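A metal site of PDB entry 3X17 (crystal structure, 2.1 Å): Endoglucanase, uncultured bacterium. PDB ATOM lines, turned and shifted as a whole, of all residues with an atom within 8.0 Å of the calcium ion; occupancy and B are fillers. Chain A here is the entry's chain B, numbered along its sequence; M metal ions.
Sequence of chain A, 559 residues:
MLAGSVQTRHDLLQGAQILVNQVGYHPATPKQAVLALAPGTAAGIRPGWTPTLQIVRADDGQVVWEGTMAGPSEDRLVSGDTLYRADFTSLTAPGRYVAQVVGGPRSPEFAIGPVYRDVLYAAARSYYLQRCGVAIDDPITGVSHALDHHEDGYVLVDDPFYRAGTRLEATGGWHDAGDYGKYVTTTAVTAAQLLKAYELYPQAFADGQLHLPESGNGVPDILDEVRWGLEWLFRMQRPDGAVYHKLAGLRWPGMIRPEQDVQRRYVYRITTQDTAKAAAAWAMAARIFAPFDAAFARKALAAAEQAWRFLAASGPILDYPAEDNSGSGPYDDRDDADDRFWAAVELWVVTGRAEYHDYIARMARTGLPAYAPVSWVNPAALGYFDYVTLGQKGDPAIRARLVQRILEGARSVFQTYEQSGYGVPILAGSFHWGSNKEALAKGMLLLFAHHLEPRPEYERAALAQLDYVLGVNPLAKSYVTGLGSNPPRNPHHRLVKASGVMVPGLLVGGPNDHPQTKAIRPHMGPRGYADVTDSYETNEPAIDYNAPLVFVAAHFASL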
ATOM      1  N   ALA A 206     -14.876  11.880 -10.029  1.00  0.00           N
ATOM      2  CA  ALA A 206     -14.780  13.326  -9.861  1.00  0.00           C
ATOM      3  C   ALA A 206     -15.300  14.132 -11.066  1.00  0.00           C
ATOM      4  O   ALA A 206     -15.299  13.645 -12.194  1.00  0.00           O
ATOM      5  CB  ALA A 206     -13.327  13.731  -9.494  1.00  0.00           C
ATOM      6  N   ASP A 207     -15.653  15.389 -10.817  1.00  0.00           N
ATOM      7  CA  ASP A 207     -15.703  16.376 -11.894  1.00  0.00           C
ATOM      8  C   ASP A 207     -14.381  16.362 -12.644  1.00  0.00           C
ATOM      9  O   ASP A 207     -13.312  16.278 -12.023  1.00  0.00           O
ATOM     10  CB  ASP A 207     -16.010  17.777 -11.332  1.00  0.00           C
ATOM     11  CG  ASP A 207     -16.313  18.790 -12.417  1.00  0.00           C
ATOM     12  OD1 ASP A 207     -16.546  18.400 -13.580  1.00  0.00           O
ATOM     13  OD2 ASP A 207     -16.278  20.002 -12.122  1.00  0.00           O
ATOM     14  N   GLY A 208     -14.460  16.333 -13.978  1.00  0.00           N
ATOM     15  CA  GLY A 208     -13.287  16.393 -14.850  1.00  0.00           C
ATOM     16  C   GLY A 208     -12.610  15.056 -15.030  1.00  0.00           C
ATOM     17  O   GLY A 208     -11.733  14.919 -15.878  1.00  0.00           O
ATOM     18  N   GLN A 209     -13.020  14.056 -14.265  1.00  0.00           N
ATOM     19  CA  GLN A 209     -12.460  12.697 -14.403  1.00  0.00           C
ATOM     20  C   GLN A 209     -12.355  12.169 -15.849  1.00  0.00           C
ATOM     21  O   GLN A 209     -11.363  11.505 -16.202  1.00  0.00           O
ATOM     22  CB  GLN A 209     -13.214  11.687 -13.558  1.00  0.00           C
ATOM     23  CG  GLN A 209     -12.629  10.248 -13.677  1.00  0.00           C
ATOM     24  CD  GLN A 209     -13.540   9.210 -13.056  1.00  0.00           C
ATOM     25  OE1 GLN A 209     -14.731   9.456 -12.864  1.00  0.00           O
ATOM     26  NE2 GLN A 209     -12.981   8.055 -12.706  1.00  0.00           N
ATOM     27  N   LEU A 210     -13.356  12.444 -16.677  1.00  0.00           N
ATOM     28  CA  LEU A 210     -13.537  11.664 -17.886  1.00  0.00           C
ATOM     29  C   LEU A 210     -13.198  12.450 -19.149  1.00  0.00           C
ATOM     30  O   LEU A 210     -13.439  11.974 -20.268  1.00  0.00           O
ATOM     31  CB  LEU A 210     -14.969  11.096 -17.961  1.00  0.00           C
ATOM     32  CG  LEU A 210     -15.268  10.088 -16.860  1.00  0.00           C
ATOM     33  CD1 LEU A 210     -16.748   9.611 -16.863  1.00  0.00           C
ATOM     34  CD2 LEU A 210     -14.286   8.914 -16.956  1.00  0.00           C
ATOM     35  N   LEU A 212     -14.524  15.187 -20.596  1.00  0.00           N
ATOM     36  CA  LEU A 212     -15.744  15.316 -21.374  1.00  0.00           C
ATOM     37  C   LEU A 212     -16.000  16.793 -21.751  1.00  0.00           C
ATOM     38  O   LEU A 212     -15.418  17.698 -21.156  1.00  0.00           O
ATOM     39  CB  LEU A 212     -16.925  14.813 -20.532  1.00  0.00           C
ATOM     40  CG  LEU A 212     -16.945  13.343 -20.106  1.00  0.00           C
ATOM     41  CD1 LEU A 212     -18.202  13.043 -19.313  1.00  0.00           C
ATOM     42  CD2 LEU A 212     -16.881  12.440 -21.315  1.00  0.00           C
ATOM     43  N   PRO A 213     -16.974  17.041 -22.631  1.00  0.00           N
ATOM     44  CA  PRO A 213     -17.442  18.414 -22.819  1.00  0.00           C
ATOM     45  C   PRO A 213     -17.979  19.009 -21.520  1.00  0.00           C
ATOM     46  O   PRO A 213     -17.940  20.229 -21.321  1.00  0.00           O
ATOM     47  CB  PRO A 213     -18.591  18.271 -23.835  1.00  0.00           C
ATOM     48  CG  PRO A 213     -18.311  16.978 -24.535  1.00  0.00           C
ATOM     49  CD  PRO A 213     -17.738  16.082 -23.456  1.00  0.00           C
ATOM     50  N   GLU A 214     -18.489  18.145 -20.629  1.00  0.00           N
ATOM     51  CA  GLU A 214     -19.042  18.617 -19.362  1.00  0.00           C
ATOM     52  C   GLU A 214     -18.021  18.663 -18.209  1.00  0.00           C
ATOM     53  O   GLU A 214     -18.372  19.005 -17.077  1.00  0.00           O
ATOM     54  CB  GLU A 214     -20.307  17.805 -18.986  1.00  0.00           C
ATOM     55  CG  GLU A 214     -21.400  17.756 -20.116  1.00  0.00           C
ATOM     56  CD  GLU A 214     -21.273  16.563 -21.104  1.00  0.00           C
ATOM     57  OE1 GLU A 214     -20.227  15.881 -21.178  1.00  0.00           O
ATOM     58  OE2 GLU A 214     -22.236  16.300 -21.844  1.00  0.00           O
ATOM     59  N   SER A 215     -16.780  18.285 -18.482  1.00  0.00           N
ATOM     60  CA  SER A 215     -15.739  18.295 -17.469  1.00  0.00           C
ATOM     61  C   SER A 215     -15.561  19.730 -16.947  1.00  0.00           C
ATOM     62  O   SER A 215     -15.319  20.639 -17.714  1.00  0.00           O
ATOM     63  CB  SER A 215     -14.417  17.820 -18.073  1.00  0.00           C
ATOM     64  OG  SER A 215     -14.418  16.427 -18.315  1.00  0.00           O
ATOM     65  N   GLY A 216     -15.722  19.919 -15.645  1.00  0.00           N
ATOM     66  CA  GLY A 216     -15.464  21.231 -15.051  1.00  0.00           C
ATOM     67  C   GLY A 216     -16.725  22.044 -14.824  1.00  0.00           C
ATOM     68  O   GLY A 216     -16.645  23.220 -14.525  1.00  0.00           O
ATOM     69  N   ASN A 217     -17.893  21.399 -14.898  1.00  0.00           N
ATOM     70  CA  ASN A 217     -19.149  22.042 -14.578  1.00  0.00           C
ATOM     71  C   ASN A 217     -19.537  21.837 -13.117  1.00  0.00           C
ATOM     72  O   ASN A 217     -20.639  22.191 -12.716  1.00  0.00           O
ATOM     73  CB  ASN A 217     -20.266  21.486 -15.464  1.00  0.00           C
ATOM     74  CG  ASN A 217     -20.549  20.008 -15.180  1.00  0.00           C
ATOM     75  OD1 ASN A 217     -19.863  19.395 -14.345  1.00  0.00           O
ATOM     76  ND2 ASN A 217     -21.522  19.442 -15.864  1.00  0.00           N
ATOM     77  N   GLY A 218     -18.659  21.238 -12.321  1.00  0.00           N
ATOM     78  CA  GLY A 218     -18.941  21.043 -10.906  1.00  0.00           C
ATOM     79  C   GLY A 218     -19.711  19.769 -10.570  1.00  0.00           C
ATOM     80  O   GLY A 218     -20.071  19.544  -9.411  1.00  0.00           O
ATOM     81  N   VAL A 219     -19.962  18.934 -11.579  1.00  0.00           N
ATOM     82  CA  VAL A 219     -20.711  17.679 -11.408  1.00  0.00           C
ATOM     83  C   VAL A 219     -19.808  16.481 -11.802  1.00  0.00           C
ATOM     84  O   VAL A 219     -19.147  16.509 -12.836  1.00  0.00           O
ATOM     85  CB  VAL A 219     -22.006  17.715 -12.267  1.00  0.00           C
ATOM     86  CG1 VAL A 219     -22.837  16.441 -12.093  1.00  0.00           C
ATOM     87  CG2 VAL A 219     -22.869  18.985 -11.971  1.00  0.00           C
ATOM     88  N   PRO A 220     -19.795  15.410 -10.991  1.00  0.00           N
ATOM     89  CA  PRO A 220     -18.999  14.264 -11.406  1.00  0.00           C
ATOM     90  C   PRO A 220     -19.311  13.849 -12.838  1.00  0.00           C
ATOM     91  O   PRO A 220     -20.485  13.780 -13.202  1.00  0.00           O
ATOM     92  CB  PRO A 220     -19.441  13.168 -10.431  1.00  0.00           C
ATOM     93  CG  PRO A 220     -19.832  13.981  -9.176  1.00  0.00           C
ATOM     94  CD  PRO A 220     -20.597  15.119  -9.801  1.00  0.00           C
ATOM     95  N   ASP A 221     -18.286  13.637 -13.640  1.00  0.00           N
ATOM     96  CA  ASP A 221     -18.433  13.390 -15.070  1.00  0.00           C
ATOM     97  C   ASP A 221     -19.300  12.170 -15.330  1.00  0.00           C
ATOM     98  O   ASP A 221     -20.015  12.131 -16.314  1.00  0.00           O
ATOM     99  CB  ASP A 221     -17.056  13.205 -15.725  1.00  0.00           C
ATOM    100  CG  ASP A 221     -16.349  14.512 -15.964  1.00  0.00           C
ATOM    101  OD1 ASP A 221     -16.903  15.548 -15.558  1.00  0.00           O
ATOM    102  OD2 ASP A 221     -15.230  14.514 -16.516  1.00  0.00           O
ATOM    103  N   ILE A 222     -19.187  11.142 -14.490  1.00  0.00           N
ATOM    104  CA  ILE A 222     -19.997   9.935 -14.674  1.00  0.00           C
ATOM    105  C   ILE A 222     -21.484  10.321 -14.653  1.00  0.00           C
ATOM    106  O   ILE A 222     -22.272   9.790 -15.428  1.00  0.00           O
ATOM    107  CB  ILE A 222     -19.726   8.840 -13.595  1.00  0.00           C
ATOM    108  CG1 ILE A 222     -20.470   7.517 -13.941  1.00  0.00           C
ATOM    109  CG2 ILE A 222     -20.204   9.306 -12.246  1.00  0.00           C
ATOM    110  CD1 ILE A 222     -20.032   6.873 -15.256  1.00  0.00           C
ATOM    111  N   LEU A 223     -21.824  11.342 -13.864  1.00  0.00           N
ATOM    112  CA  LEU A 223     -23.206  11.843 -13.825  1.00  0.00           C
ATOM    113  C   LEU A 223     -23.589  12.685 -15.046  1.00  0.00           C
ATOM    114  O   LEU A 223     -24.682  12.565 -15.561  1.00  0.00           O
ATOM    115  CB  LEU A 223     -23.488  12.629 -12.531  1.00  0.00           C
ATOM    116  CG  LEU A 223     -23.321  11.819 -11.235  1.00  0.00           C
ATOM    117  CD1 LEU A 223     -23.763  12.629 -10.028  1.00  0.00           C
ATOM    118  CD2 LEU A 223     -24.065  10.489 -11.330  1.00  0.00           C
ATOM    119  N   ASP A 224     -22.643  13.455 -15.563  1.00  0.00           N
ATOM    120  CA  ASP A 224     -22.854  14.072 -16.870  1.00  0.00           C
ATOM    121  C   ASP A 224     -23.108  13.019 -17.943  1.00  0.00           C
ATOM    122  O   ASP A 224     -23.978  13.197 -18.786  1.00  0.00           O
ATOM    123  CB  ASP A 224     -21.677  14.952 -17.270  1.00  0.00           C
ATOM    124  CG  ASP A 224     -21.534  16.163 -16.367  1.00  0.00           C
ATOM    125  OD1 ASP A 224     -22.553  16.842 -16.090  1.00  0.00           O
ATOM    126  OD2 ASP A 224     -20.424  16.335 -15.832  1.00  0.00           O
ATOM    127  N   GLU A 225     -22.356  11.917 -17.907  1.00  0.00           N
ATOM    128  CA  GLU A 225     -22.582  10.900 -18.946  1.00  0.00           C
ATOM    129  C   GLU A 225     -23.982  10.310 -18.796  1.00  0.00           C
ATOM    130  O   GLU A 225     -24.716  10.196 -19.770  1.00  0.00           O
ATOM    131  CB  GLU A 225     -21.538   9.791 -18.900  1.00  0.00           C
ATOM    132  CG  GLU A 225     -21.607   8.895 -20.168  1.00  0.00           C
ATOM    133  CD  GLU A 225     -21.217   9.680 -21.429  1.00  0.00           C
ATOM    134  OE1 GLU A 225     -20.237  10.451 -21.360  1.00  0.00           O
ATOM    135  OE2 GLU A 225     -21.933   9.580 -22.453  1.00  0.00           O
HETATM  136 CA    CA M   1     -18.472  17.442 -14.850  1.00  0.00          CA
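Ser 215 touches the calcium ion. Gly 216 touches the calcium ion (N to CA, 3.8 Å). Eight residues have an atom within 4 Å of the calcium ion: Asp 207, Glu 214, Ser 215, Gly 216, Asn 217, Val 219, Asp 221 and Asp 224. The nearest printed residue that does not touch the calcium ion is Pro 220 (4.2 Å).
O of Val 219 binds the calcium ion (2.3 Å). The calcium ion is bound by OD2 of Asp 224 (2.4 Å). The side-chain amide oxygen (OD1) of Asn 217 is bound to the calcium ion (2.5 Å). The calcium ion is bound by the side-chain carboxylate (OD1) of Asp 207, 2.5 Å away. The calcium ion is bound by OD1 of Asp 221 (2.6 Å). O of Glu 214 binds the calcium ion. The calcium ion has six donor atoms within binding distance.
OD1 of Asp 207 lies close to N of Gly 216 (2.7 Å). The side-chain carboxylate of Asp 207 sits at hydrogen-bond distance from the backbone NH of Gly 218 (2.7 Å). The side-chain carboxylate (OD2) of Asp 221 lies within hydrogen-bond range of the side-chain hydroxyl (OG) of Ser 215, 2.7 Å away. OD2 of Asp 221 sits close to N of Gly 208 (3.2 Å). O of Ala 206 is in hydrogen-bond range of N of Asp 221, at 3.3 Å. N of Gln 209 is in hydrogen-bond range of OD2 of Asp 221 (3.2 Å). OD2 of Asp 221 is in hydrogen-bond range of N of Leu 210 (2.8 Å). OG of Ser 215 sits at hydrogen-bond distance from N of Leu 212, at 2.6 Å.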
